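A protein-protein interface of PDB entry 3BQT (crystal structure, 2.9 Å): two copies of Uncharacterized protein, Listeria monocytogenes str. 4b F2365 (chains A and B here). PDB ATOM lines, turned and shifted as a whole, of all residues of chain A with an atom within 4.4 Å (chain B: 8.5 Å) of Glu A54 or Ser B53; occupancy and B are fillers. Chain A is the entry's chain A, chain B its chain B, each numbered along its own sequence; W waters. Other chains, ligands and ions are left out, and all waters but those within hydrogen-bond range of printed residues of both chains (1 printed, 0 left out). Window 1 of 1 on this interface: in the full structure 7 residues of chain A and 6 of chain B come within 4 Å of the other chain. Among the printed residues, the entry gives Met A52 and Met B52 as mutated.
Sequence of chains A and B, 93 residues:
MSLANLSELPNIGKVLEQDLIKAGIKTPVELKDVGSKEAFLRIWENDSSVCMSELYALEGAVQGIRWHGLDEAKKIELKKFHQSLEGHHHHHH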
ATOM      1  N   LEU A  16      17.341  -0.743 -11.497  1.00  0.00           N
ATOM      2  CA  LEU A  16      17.813   0.557 -11.837  1.00  0.00           C
ATOM      3  C   LEU A  16      17.905   0.469 -13.365  1.00  0.00           C
ATOM      4  O   LEU A  16      17.418   1.364 -14.087  1.00  0.00           O
ATOM      5  CB  LEU A  16      19.133   0.730 -11.201  1.00  0.00           C
ATOM      6  CG  LEU A  16      19.795   2.060 -11.391  1.00  0.00           C
ATOM      7  CD1 LEU A  16      19.047   3.107 -10.622  1.00  0.00           C
ATOM      8  CD2 LEU A  16      21.229   1.967 -10.896  1.00  0.00           C
ATOM      9  N   VAL A  50      12.215   7.461  -7.351  1.00  0.00           N
ATOM     10  CA  VAL A  50      13.659   7.287  -7.461  1.00  0.00           C
ATOM     11  C   VAL A  50      14.209   8.121  -6.330  1.00  0.00           C
ATOM     12  O   VAL A  50      13.466   8.902  -5.738  1.00  0.00           O
ATOM     13  CB  VAL A  50      14.173   7.815  -8.775  1.00  0.00           C
ATOM     14  CG1 VAL A  50      15.688   7.794  -8.818  1.00  0.00           C
ATOM     15  CG2 VAL A  50      13.614   6.964  -9.847  1.00  0.00           C
ATOM     16  N   CYS A  51      15.489   7.997  -6.011  1.00  0.00           N
ATOM     17  CA  CYS A  51      15.971   8.793  -4.911  1.00  0.00           C
ATOM     18  C   CYS A  51      17.476   8.843  -4.849  1.00  0.00           C
ATOM     19  O   CYS A  51      18.161   8.280  -5.699  1.00  0.00           O
ATOM     20  CB  CYS A  51      15.366   8.227  -3.638  1.00  0.00           C
ATOM     21  SG  CYS A  51      15.917   8.821  -2.007  1.00  0.00           S
ATOM     22  N   MET A  52      17.977   9.574  -3.864  1.00  0.00           N
ATOM     23  CA  MET A  52      19.399   9.740  -3.631  1.00  0.00           C
ATOM     24  C   MET A  52      20.250   8.504  -3.897  1.00  0.00           C
ATOM     25  O   MET A  52      21.352   8.612  -4.432  1.00  0.00           O
ATOM     26  CB  MET A  52      19.591  10.208  -2.205  1.00  0.00           C
ATOM     27  CG  MET A  52      19.533  11.696  -2.078  1.00  0.00           C
ATOM     28  SD  MET A  52      21.172  12.458  -2.740  1.00  0.00           S
ATOM     29  CE  MET A  52      22.240  12.075  -1.205  1.00  0.00           C
ATOM     30  N   SER A  53      19.749   7.340  -3.489  1.00  0.00           N
ATOM     31  CA  SER A  53      20.434   6.071  -3.711  1.00  0.00           C
ATOM     32  C   SER A  53      20.787   5.955  -5.180  1.00  0.00           C
ATOM     33  O   SER A  53      21.949   5.792  -5.561  1.00  0.00           O
ATOM     34  CB  SER A  53      19.518   4.900  -3.381  1.00  0.00           C
ATOM     35  OG  SER A  53      19.598   4.526  -2.028  1.00  0.00           O
ATOM     36  N   GLU A  54      19.755   6.029  -6.009  1.00  0.00           N
ATOM     37  CA  GLU A  54      19.938   5.912  -7.429  1.00  0.00           C
ATOM     38  C   GLU A  54      20.845   6.980  -8.003  1.00  0.00           C
ATOM     39  O   GLU A  54      21.578   6.706  -8.948  1.00  0.00           O
ATOM     40  CB  GLU A  54      18.582   5.913  -8.111  1.00  0.00           C
ATOM     41  CG  GLU A  54      17.810   4.631  -7.890  1.00  0.00           C
ATOM     42  CD  GLU A  54      17.435   4.364  -6.428  1.00  0.00           C
ATOM     43  OE1 GLU A  54      16.618   5.122  -5.859  1.00  0.00           O
ATOM     44  OE2 GLU A  54      17.951   3.379  -5.847  1.00  0.00           O
ATOM     45  N   LEU A  55      20.805   8.186  -7.438  1.00  0.00           N
ATOM     46  CA  LEU A  55      21.655   9.274  -7.920  1.00  0.00           C
ATOM     47  C   LEU A  55      23.123   8.891  -7.806  1.00  0.00           C
ATOM     48  O   LEU A  55      23.888   8.986  -8.768  1.00  0.00           O
ATOM     49  CB  LEU A  55      21.407  10.539  -7.113  1.00  0.00           C
ATOM     50  CG  LEU A  55      21.243  11.798  -7.955  1.00  0.00           C
ATOM     51  CD1 LEU A  55      21.053  13.000  -7.063  1.00  0.00           C
ATOM     52  CD2 LEU A  55      22.454  11.979  -8.807  1.00  0.00           C
ATOM     53  N   TYR A  56      23.495   8.453  -6.610  1.00  0.00           N
ATOM     54  CA  TYR A  56      24.847   8.016  -6.300  1.00  0.00           C
ATOM     55  C   TYR A  56      25.222   6.820  -7.140  1.00  0.00           C
ATOM     56  O   TYR A  56      26.328   6.722  -7.673  1.00  0.00           O
ATOM     57  CB  TYR A  56      24.934   7.635  -4.831  1.00  0.00           C
ATOM     58  CG  TYR A  56      24.923   8.818  -3.905  1.00  0.00           C
ATOM     59  CD1 TYR A  56      25.325  10.064  -4.357  1.00  0.00           C
ATOM     60  CD2 TYR A  56      24.609   8.673  -2.560  1.00  0.00           C
ATOM     61  CE1 TYR A  56      25.433  11.135  -3.501  1.00  0.00           C
ATOM     62  CE2 TYR A  56      24.714   9.732  -1.688  1.00  0.00           C
ATOM     63  CZ  TYR A  56      25.130  10.966  -2.167  1.00  0.00           C
ATOM     64  OH  TYR A  56      25.274  12.021  -1.291  1.00  0.00           O
ATOM     65  N   ALA A  57      24.271   5.906  -7.247  1.00  0.00           N
ATOM     66  CA  ALA A  57      24.460   4.711  -8.031  1.00  0.00           C
ATOM     67  C   ALA A  57      24.818   5.123  -9.452  1.00  0.00           C
ATOM     68  O   ALA A  57      25.751   4.586 -10.032  1.00  0.00           O
ATOM     69  CB  ALA A  57      23.179   3.856  -8.010  1.00  0.00           C
ATOM     70  N   LEU A  58      24.107   6.103 -10.002  1.00  0.00           N
ATOM     71  CA  LEU A  58      24.378   6.536 -11.366  1.00  0.00           C
ATOM     72  C   LEU A  58      25.723   7.206 -11.571  1.00  0.00           C
ATOM     73  O   LEU A  58      26.411   6.935 -12.548  1.00  0.00           O
ATOM     74  CB  LEU A  58      23.257   7.445 -11.859  1.00  0.00           C
ATOM     75  CG  LEU A  58      22.035   6.605 -12.205  1.00  0.00           C
ATOM     76  CD1 LEU A  58      21.004   7.426 -12.913  1.00  0.00           C
ATOM     77  CD2 LEU A  58      22.490   5.456 -13.100  1.00  0.00           C
ATOM     78  N   ASN B  11      21.916  -6.795   0.263  1.00  0.00           N
ATOM     79  CA  ASN B  11      21.420  -5.449   0.007  1.00  0.00           C
ATOM     80  C   ASN B  11      21.899  -4.352   0.953  1.00  0.00           C
ATOM     81  O   ASN B  11      21.450  -3.216   0.865  1.00  0.00           O
ATOM     82  CB  ASN B  11      19.888  -5.438   0.003  1.00  0.00           C
ATOM     83  CG  ASN B  11      19.289  -6.590  -0.770  1.00  0.00           C
ATOM     84  OD1 ASN B  11      18.668  -7.478  -0.201  1.00  0.00           O
ATOM     85  ND2 ASN B  11      19.468  -6.578  -2.070  1.00  0.00           N
ATOM     86  N   LEU B  16      24.096   2.165   4.794  1.00  0.00           N
ATOM     87  CA  LEU B  16      22.820   1.654   5.312  1.00  0.00           C
ATOM     88  C   LEU B  16      23.190   1.025   6.661  1.00  0.00           C
ATOM     89  O   LEU B  16      22.478   1.176   7.668  1.00  0.00           O
ATOM     90  CB  LEU B  16      22.282   0.519   4.448  1.00  0.00           C
ATOM     91  CG  LEU B  16      20.913  -0.028   4.882  1.00  0.00           C
ATOM     92  CD1 LEU B  16      19.868   1.033   4.680  1.00  0.00           C
ATOM     93  CD2 LEU B  16      20.563  -1.250   4.063  1.00  0.00           C
ATOM     94  N   PHE B  40      13.394   0.719   9.361  1.00  0.00           N
ATOM     95  CA  PHE B  40      13.335   1.840   8.428  1.00  0.00           C
ATOM     96  C   PHE B  40      12.687   3.056   9.053  1.00  0.00           C
ATOM     97  O   PHE B  40      13.161   4.181   8.904  1.00  0.00           O
ATOM     98  CB  PHE B  40      12.516   1.399   7.225  1.00  0.00           C
ATOM     99  CG  PHE B  40      12.307   2.455   6.224  1.00  0.00           C
ATOM    100  CD1 PHE B  40      13.268   2.707   5.248  1.00  0.00           C
ATOM    101  CD2 PHE B  40      11.133   3.197   6.224  1.00  0.00           C
ATOM    102  CE1 PHE B  40      13.050   3.686   4.269  1.00  0.00           C
ATOM    103  CE2 PHE B  40      10.911   4.176   5.248  1.00  0.00           C
ATOM    104  CZ  PHE B  40      11.869   4.417   4.277  1.00  0.00           C
ATOM    105  N   VAL B  50      15.066   9.295   3.663  1.00  0.00           N
ATOM    106  CA  VAL B  50      15.818   8.107   3.320  1.00  0.00           C
ATOM    107  C   VAL B  50      15.016   7.261   2.348  1.00  0.00           C
ATOM    108  O   VAL B  50      13.872   6.859   2.611  1.00  0.00           O
ATOM    109  CB  VAL B  50      16.231   7.314   4.562  1.00  0.00           C
ATOM    110  CG1 VAL B  50      15.027   6.709   5.232  1.00  0.00           C
ATOM    111  CG2 VAL B  50      17.279   6.273   4.159  1.00  0.00           C
ATOM    112  N   CYS B  51      15.642   7.041   1.202  1.00  0.00           N
ATOM    113  CA  CYS B  51      15.087   6.308   0.086  1.00  0.00           C
ATOM    114  C   CYS B  51      14.235   5.057   0.312  1.00  0.00           C
ATOM    115  O   CYS B  51      14.426   4.288   1.255  1.00  0.00           O
ATOM    116  CB  CYS B  51      16.233   5.957  -0.848  1.00  0.00           C
ATOM    117  SG  CYS B  51      17.240   7.357  -1.437  1.00  0.00           S
ATOM    118  N   MET B  52      13.302   4.865  -0.607  1.00  0.00           N
ATOM    119  CA  MET B  52      12.429   3.715  -0.621  1.00  0.00           C
ATOM    120  C   MET B  52      13.267   2.514  -0.999  1.00  0.00           C
ATOM    121  O   MET B  52      13.015   1.391  -0.556  1.00  0.00           O
ATOM    122  CB  MET B  52      11.401   3.921  -1.679  1.00  0.00           C
ATOM    123  CG  MET B  52      10.067   4.172  -1.141  1.00  0.00           C
ATOM    124  SD  MET B  52       9.079   2.845  -2.095  1.00  0.00           S
ATOM    125  CE  MET B  52       9.358   1.311  -0.954  1.00  0.00           C
ATOM    126  N   SER B  53      14.247   2.756  -1.861  1.00  0.00           N
ATOM    127  CA  SER B  53      15.146   1.705  -2.274  1.00  0.00           C
ATOM    128  C   SER B  53      15.683   1.075  -1.007  1.00  0.00           C
ATOM    129  O   SER B  53      15.921  -0.125  -0.954  1.00  0.00           O
ATOM    130  CB  SER B  53      16.296   2.291  -3.095  1.00  0.00           C
ATOM    131  OG  SER B  53      15.947   2.369  -4.470  1.00  0.00           O
ATOM    132  N   GLU B  54      15.847   1.886   0.031  1.00  0.00           N
ATOM    133  CA  GLU B  54      16.373   1.357   1.278  1.00  0.00           C
ATOM    134  C   GLU B  54      15.330   0.588   2.130  1.00  0.00           C
ATOM    135  O   GLU B  54      15.706  -0.181   3.001  1.00  0.00           O
ATOM    136  CB  GLU B  54      17.077   2.480   2.076  1.00  0.00           C
ATOM    137  CG  GLU B  54      18.096   3.360   1.261  1.00  0.00           C
ATOM    138  CD  GLU B  54      19.291   2.608   0.609  1.00  0.00           C
ATOM    139  OE1 GLU B  54      20.428   3.143   0.701  1.00  0.00           O
ATOM    140  OE2 GLU B  54      19.099   1.514  -0.003  1.00  0.00           O
ATOM    141  N   LEU B  55      14.031   0.762   1.891  1.00  0.00           N
ATOM    142  CA  LEU B  55      13.061  -0.025   2.668  1.00  0.00           C
ATOM    143  C   LEU B  55      13.016  -1.410   2.032  1.00  0.00           C
ATOM    144  O   LEU B  55      12.870  -2.416   2.727  1.00  0.00           O
ATOM    145  CB  LEU B  55      11.642   0.585   2.669  1.00  0.00           C
ATOM    146  CG  LEU B  55      10.537  -0.223   3.391  1.00  0.00           C
ATOM    147  CD1 LEU B  55      10.704  -0.177   4.906  1.00  0.00           C
ATOM    148  CD2 LEU B  55       9.163   0.331   2.998  1.00  0.00           C
ATOM    149  N   TYR B  56      13.130  -1.467   0.711  1.00  0.00           N
ATOM    150  CA  TYR B  56      13.140  -2.753   0.040  1.00  0.00           C
ATOM    151  C   TYR B  56      14.355  -3.543   0.509  1.00  0.00           C
ATOM    152  O   TYR B  56      14.227  -4.659   1.009  1.00  0.00           O
ATOM    153  CB  TYR B  56      13.250  -2.594  -1.485  1.00  0.00           C
ATOM    154  CG  TYR B  56      12.021  -2.074  -2.195  1.00  0.00           C
ATOM    155  CD1 TYR B  56      10.764  -2.567  -1.887  1.00  0.00           C
ATOM    156  CD2 TYR B  56      12.126  -1.130  -3.217  1.00  0.00           C
ATOM    157  CE1 TYR B  56       9.627  -2.147  -2.581  1.00  0.00           C
ATOM    158  CE2 TYR B  56      11.002  -0.691  -3.916  1.00  0.00           C
ATOM    159  CZ  TYR B  56       9.751  -1.206  -3.600  1.00  0.00           C
ATOM    160  OH  TYR B  56       8.636  -0.804  -4.322  1.00  0.00           O
ATOM    161  N   ALA B  57      15.539  -2.957   0.337  1.00  0.00           N
ATOM    162  CA  ALA B  57      16.754  -3.650   0.694  1.00  0.00           C
ATOM    163  C   ALA B  57      16.724  -4.415   1.992  1.00  0.00           C
ATOM    164  O   ALA B  57      17.113  -5.583   2.040  1.00  0.00           O
ATOM    165  CB  ALA B  57      17.945  -2.713   0.639  1.00  0.00           C
ATOM    166  N   LEU B  58      16.238  -3.775   3.037  1.00  0.00           N
ATOM    167  CA  LEU B  58      16.159  -4.409   4.349  1.00  0.00           C
ATOM    168  C   LEU B  58      15.157  -5.546   4.351  1.00  0.00           C
ATOM    169  O   LEU B  58      15.457  -6.631   4.853  1.00  0.00           O
ATOM    170  CB  LEU B  58      15.709  -3.414   5.396  1.00  0.00           C
ATOM    171  CG  LEU B  58      16.508  -2.117   5.507  1.00  0.00           C
ATOM    172  CD1 LEU B  58      15.684  -1.064   6.194  1.00  0.00           C
ATOM    173  CD2 LEU B  58      17.806  -2.354   6.234  1.00  0.00           C
ATOM    174  N   GLU B  59      13.965  -5.332   3.802  1.00  0.00           N
ATOM    175  CA  GLU B  59      13.041  -6.443   3.800  1.00  0.00           C
ATOM    176  C   GLU B  59      13.723  -7.514   3.007  1.00  0.00           C
ATOM    177  O   GLU B  59      13.652  -8.675   3.357  1.00  0.00           O
ATOM    178  CB  GLU B  59      11.734  -6.090   3.162  1.00  0.00           C
ATOM    179  CG  GLU B  59      10.818  -7.308   3.093  1.00  0.00           C
ATOM    180  CD  GLU B  59      10.353  -7.806   4.454  1.00  0.00           C
ATOM    181  OE1 GLU B  59       9.729  -8.889   4.520  1.00  0.00           O
ATOM    182  OE2 GLU B  59      10.592  -7.112   5.461  1.00  0.00           O
ATOM    183  N   GLY B  60      14.432  -7.110   1.959  1.00  0.00           N
ATOM    184  CA  GLY B  60      15.155  -8.082   1.172  1.00  0.00           C
ATOM    185  C   GLY B  60      16.069  -8.787   2.142  1.00  0.00           C
ATOM    186  O   GLY B  60      16.197  -9.994   2.127  1.00  0.00           O
ATOM    187  N   TRP B  67      16.715  -7.785  -3.033  1.00  0.00           N
ATOM    188  CA  TRP B  67      15.355  -7.275  -3.131  1.00  0.00           C
ATOM    189  C   TRP B  67      14.567  -7.288  -4.431  1.00  0.00           C
ATOM    190  O   TRP B  67      13.350  -7.297  -4.390  1.00  0.00           O
ATOM    191  CB  TRP B  67      15.238  -5.889  -2.484  1.00  0.00           C
ATOM    192  CG  TRP B  67      15.967  -4.731  -3.099  1.00  0.00           C
ATOM    193  CD1 TRP B  67      17.153  -4.189  -2.681  1.00  0.00           C
ATOM    194  CD2 TRP B  67      15.486  -3.878  -4.141  1.00  0.00           C
ATOM    195  NE1 TRP B  67      17.425  -3.034  -3.383  1.00  0.00           N
ATOM    196  CE2 TRP B  67      16.409  -2.814  -4.268  1.00  0.00           C
ATOM    197  CE3 TRP B  67      14.337  -3.880  -4.942  1.00  0.00           C
ATOM    198  CZ2 TRP B  67      16.237  -1.795  -5.214  1.00  0.00           C
ATOM    199  CZ3 TRP B  67      14.169  -2.859  -5.883  1.00  0.00           C
ATOM    200  CH2 TRP B  67      15.102  -1.825  -5.993  1.00  0.00           C
ATOM    201  N   LEU B  70      11.820  -9.937  -4.524  1.00  0.00           N
ATOM    202  CA  LEU B  70      10.701  -9.908  -3.566  1.00  0.00           C
ATOM    203  C   LEU B  70       9.380 -10.102  -4.301  1.00  0.00           C
ATOM    204  O   LEU B  70       9.208  -9.545  -5.375  1.00  0.00           O
ATOM    205  CB  LEU B  70      10.631  -8.540  -2.880  1.00  0.00           C
ATOM    206  CG  LEU B  70      11.217  -8.088  -1.538  1.00  0.00           C
ATOM    207  CD1 LEU B  70      12.271  -9.024  -1.023  1.00  0.00           C
ATOM    208  CD2 LEU B  70      11.773  -6.693  -1.737  1.00  0.00           C
ATOM    209  N   HIS B  82       5.689   3.456   2.666  1.00  0.00           N
ATOM    210  CA  HIS B  82       6.610   4.559   2.544  1.00  0.00           C
ATOM    211  C   HIS B  82       5.781   5.795   2.234  1.00  0.00           C
ATOM    212  O   HIS B  82       6.036   6.877   2.759  1.00  0.00           O
ATOM    213  CB  HIS B  82       7.614   4.282   1.437  1.00  0.00           C
ATOM    214  CG  HIS B  82       8.572   5.398   1.209  1.00  0.00           C
ATOM    215  ND1 HIS B  82       8.337   6.401   0.280  1.00  0.00           N
ATOM    216  CD2 HIS B  82       9.758   5.680   1.771  1.00  0.00           C
ATOM    217  CE1 HIS B  82       9.347   7.239   0.293  1.00  0.00           C
ATOM    218  NE2 HIS B  82      10.233   6.833   1.186  1.00  0.00           N
HETATM  219  O   HOH W   1      15.088   5.332  -3.814  1.00  0.00           O
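Printed residues of chain B within 4 Å of Met A52: Cys B51.
Of chain B, only Ser B53 (2.6 Å) comes within 4 Å of Glu A54.
Phe B40 touches none of the printed residues of chain A.
Ser B53 touches just one residue of chain A: Glu A54.
Of the printed residues of chain A, Glu B54 touches Ser A53.
Leu B70 touches none of the printed residues of chain A.
The nearest residue of chain A that does not touch Ser B53 is Ser A53 (4.1 Å).
SG of Cys A51 is disulfide-bonded to SG of Cys B51.
The backbone NH of Met A52 is in hydrogen-bond range of the side-chain sulfur of Cys B51 (3.4 Å).
The side-chain sulfur (SG) of Cys B51 lies within hydrogen-bond range of the backbone NH (N) of Ser A53 (3.2 Å).
The side-chain hydroxyl (OG) of Ser A53 lies within hydrogen-bond range of the side-chain carboxylate (OE1) of Glu B54 (3.2 Å).
OE2 of Glu A54 lies within hydrogen-bond range of OG of Ser B53 (2.6 Å).
N of Cys A51 is in hydrogen-bond range of OE1 of Glu A54.
Of the 10 printed residues of chain A, 4 touch a printed residue of chain B.
Hydrophobic or aromatic side chains of chain A within 4 Å of the printed part of chain B: Met A52.
Of the 17 printed residues of chain B, 3 touch a printed residue of chain A.
Printed residues of chain B that touch a printed residue of chain A: Cys B51, Ser B53 and Glu B54.
Among the printed residues, 5 pairs touch across the chains.
Among the printed residues, no Asp or Glu carboxylate lies within 4 Å of a Lys or Arg side-chain nitrogen of the other chain.
Cys B51 touches its own counterpart, Cys A51.
Met A52 touches Cys B51, but with the chains exchanged Cys A51 does not touch Met B52 (4.9 Å).
Ser A53 touches Cys B51, but with the chains exchanged Cys A51 does not touch Ser B53 (5.9 Å).
Ser A53 touches Glu B54, and with the chains exchanged Glu A54 touches Ser B53.
Positions printed for both chains: 16, 50, 51, 52, 53, 54, 55, 56, 57 and 58.
Of the 5 pairs that touch across the chains among the printed residues, 3 have their exchanged pair printed and touching as well.
Water W1 lies within hydrogen-bond range of the side-chain carboxylate of Glu A54 (2.6 Å), the side-chain hydroxyl of Ser B53 (3.2 Å), the backbone NH of Cys A51 (3.5 Å) and the side-chain sulfur of Cys B51 (3.8 Å).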
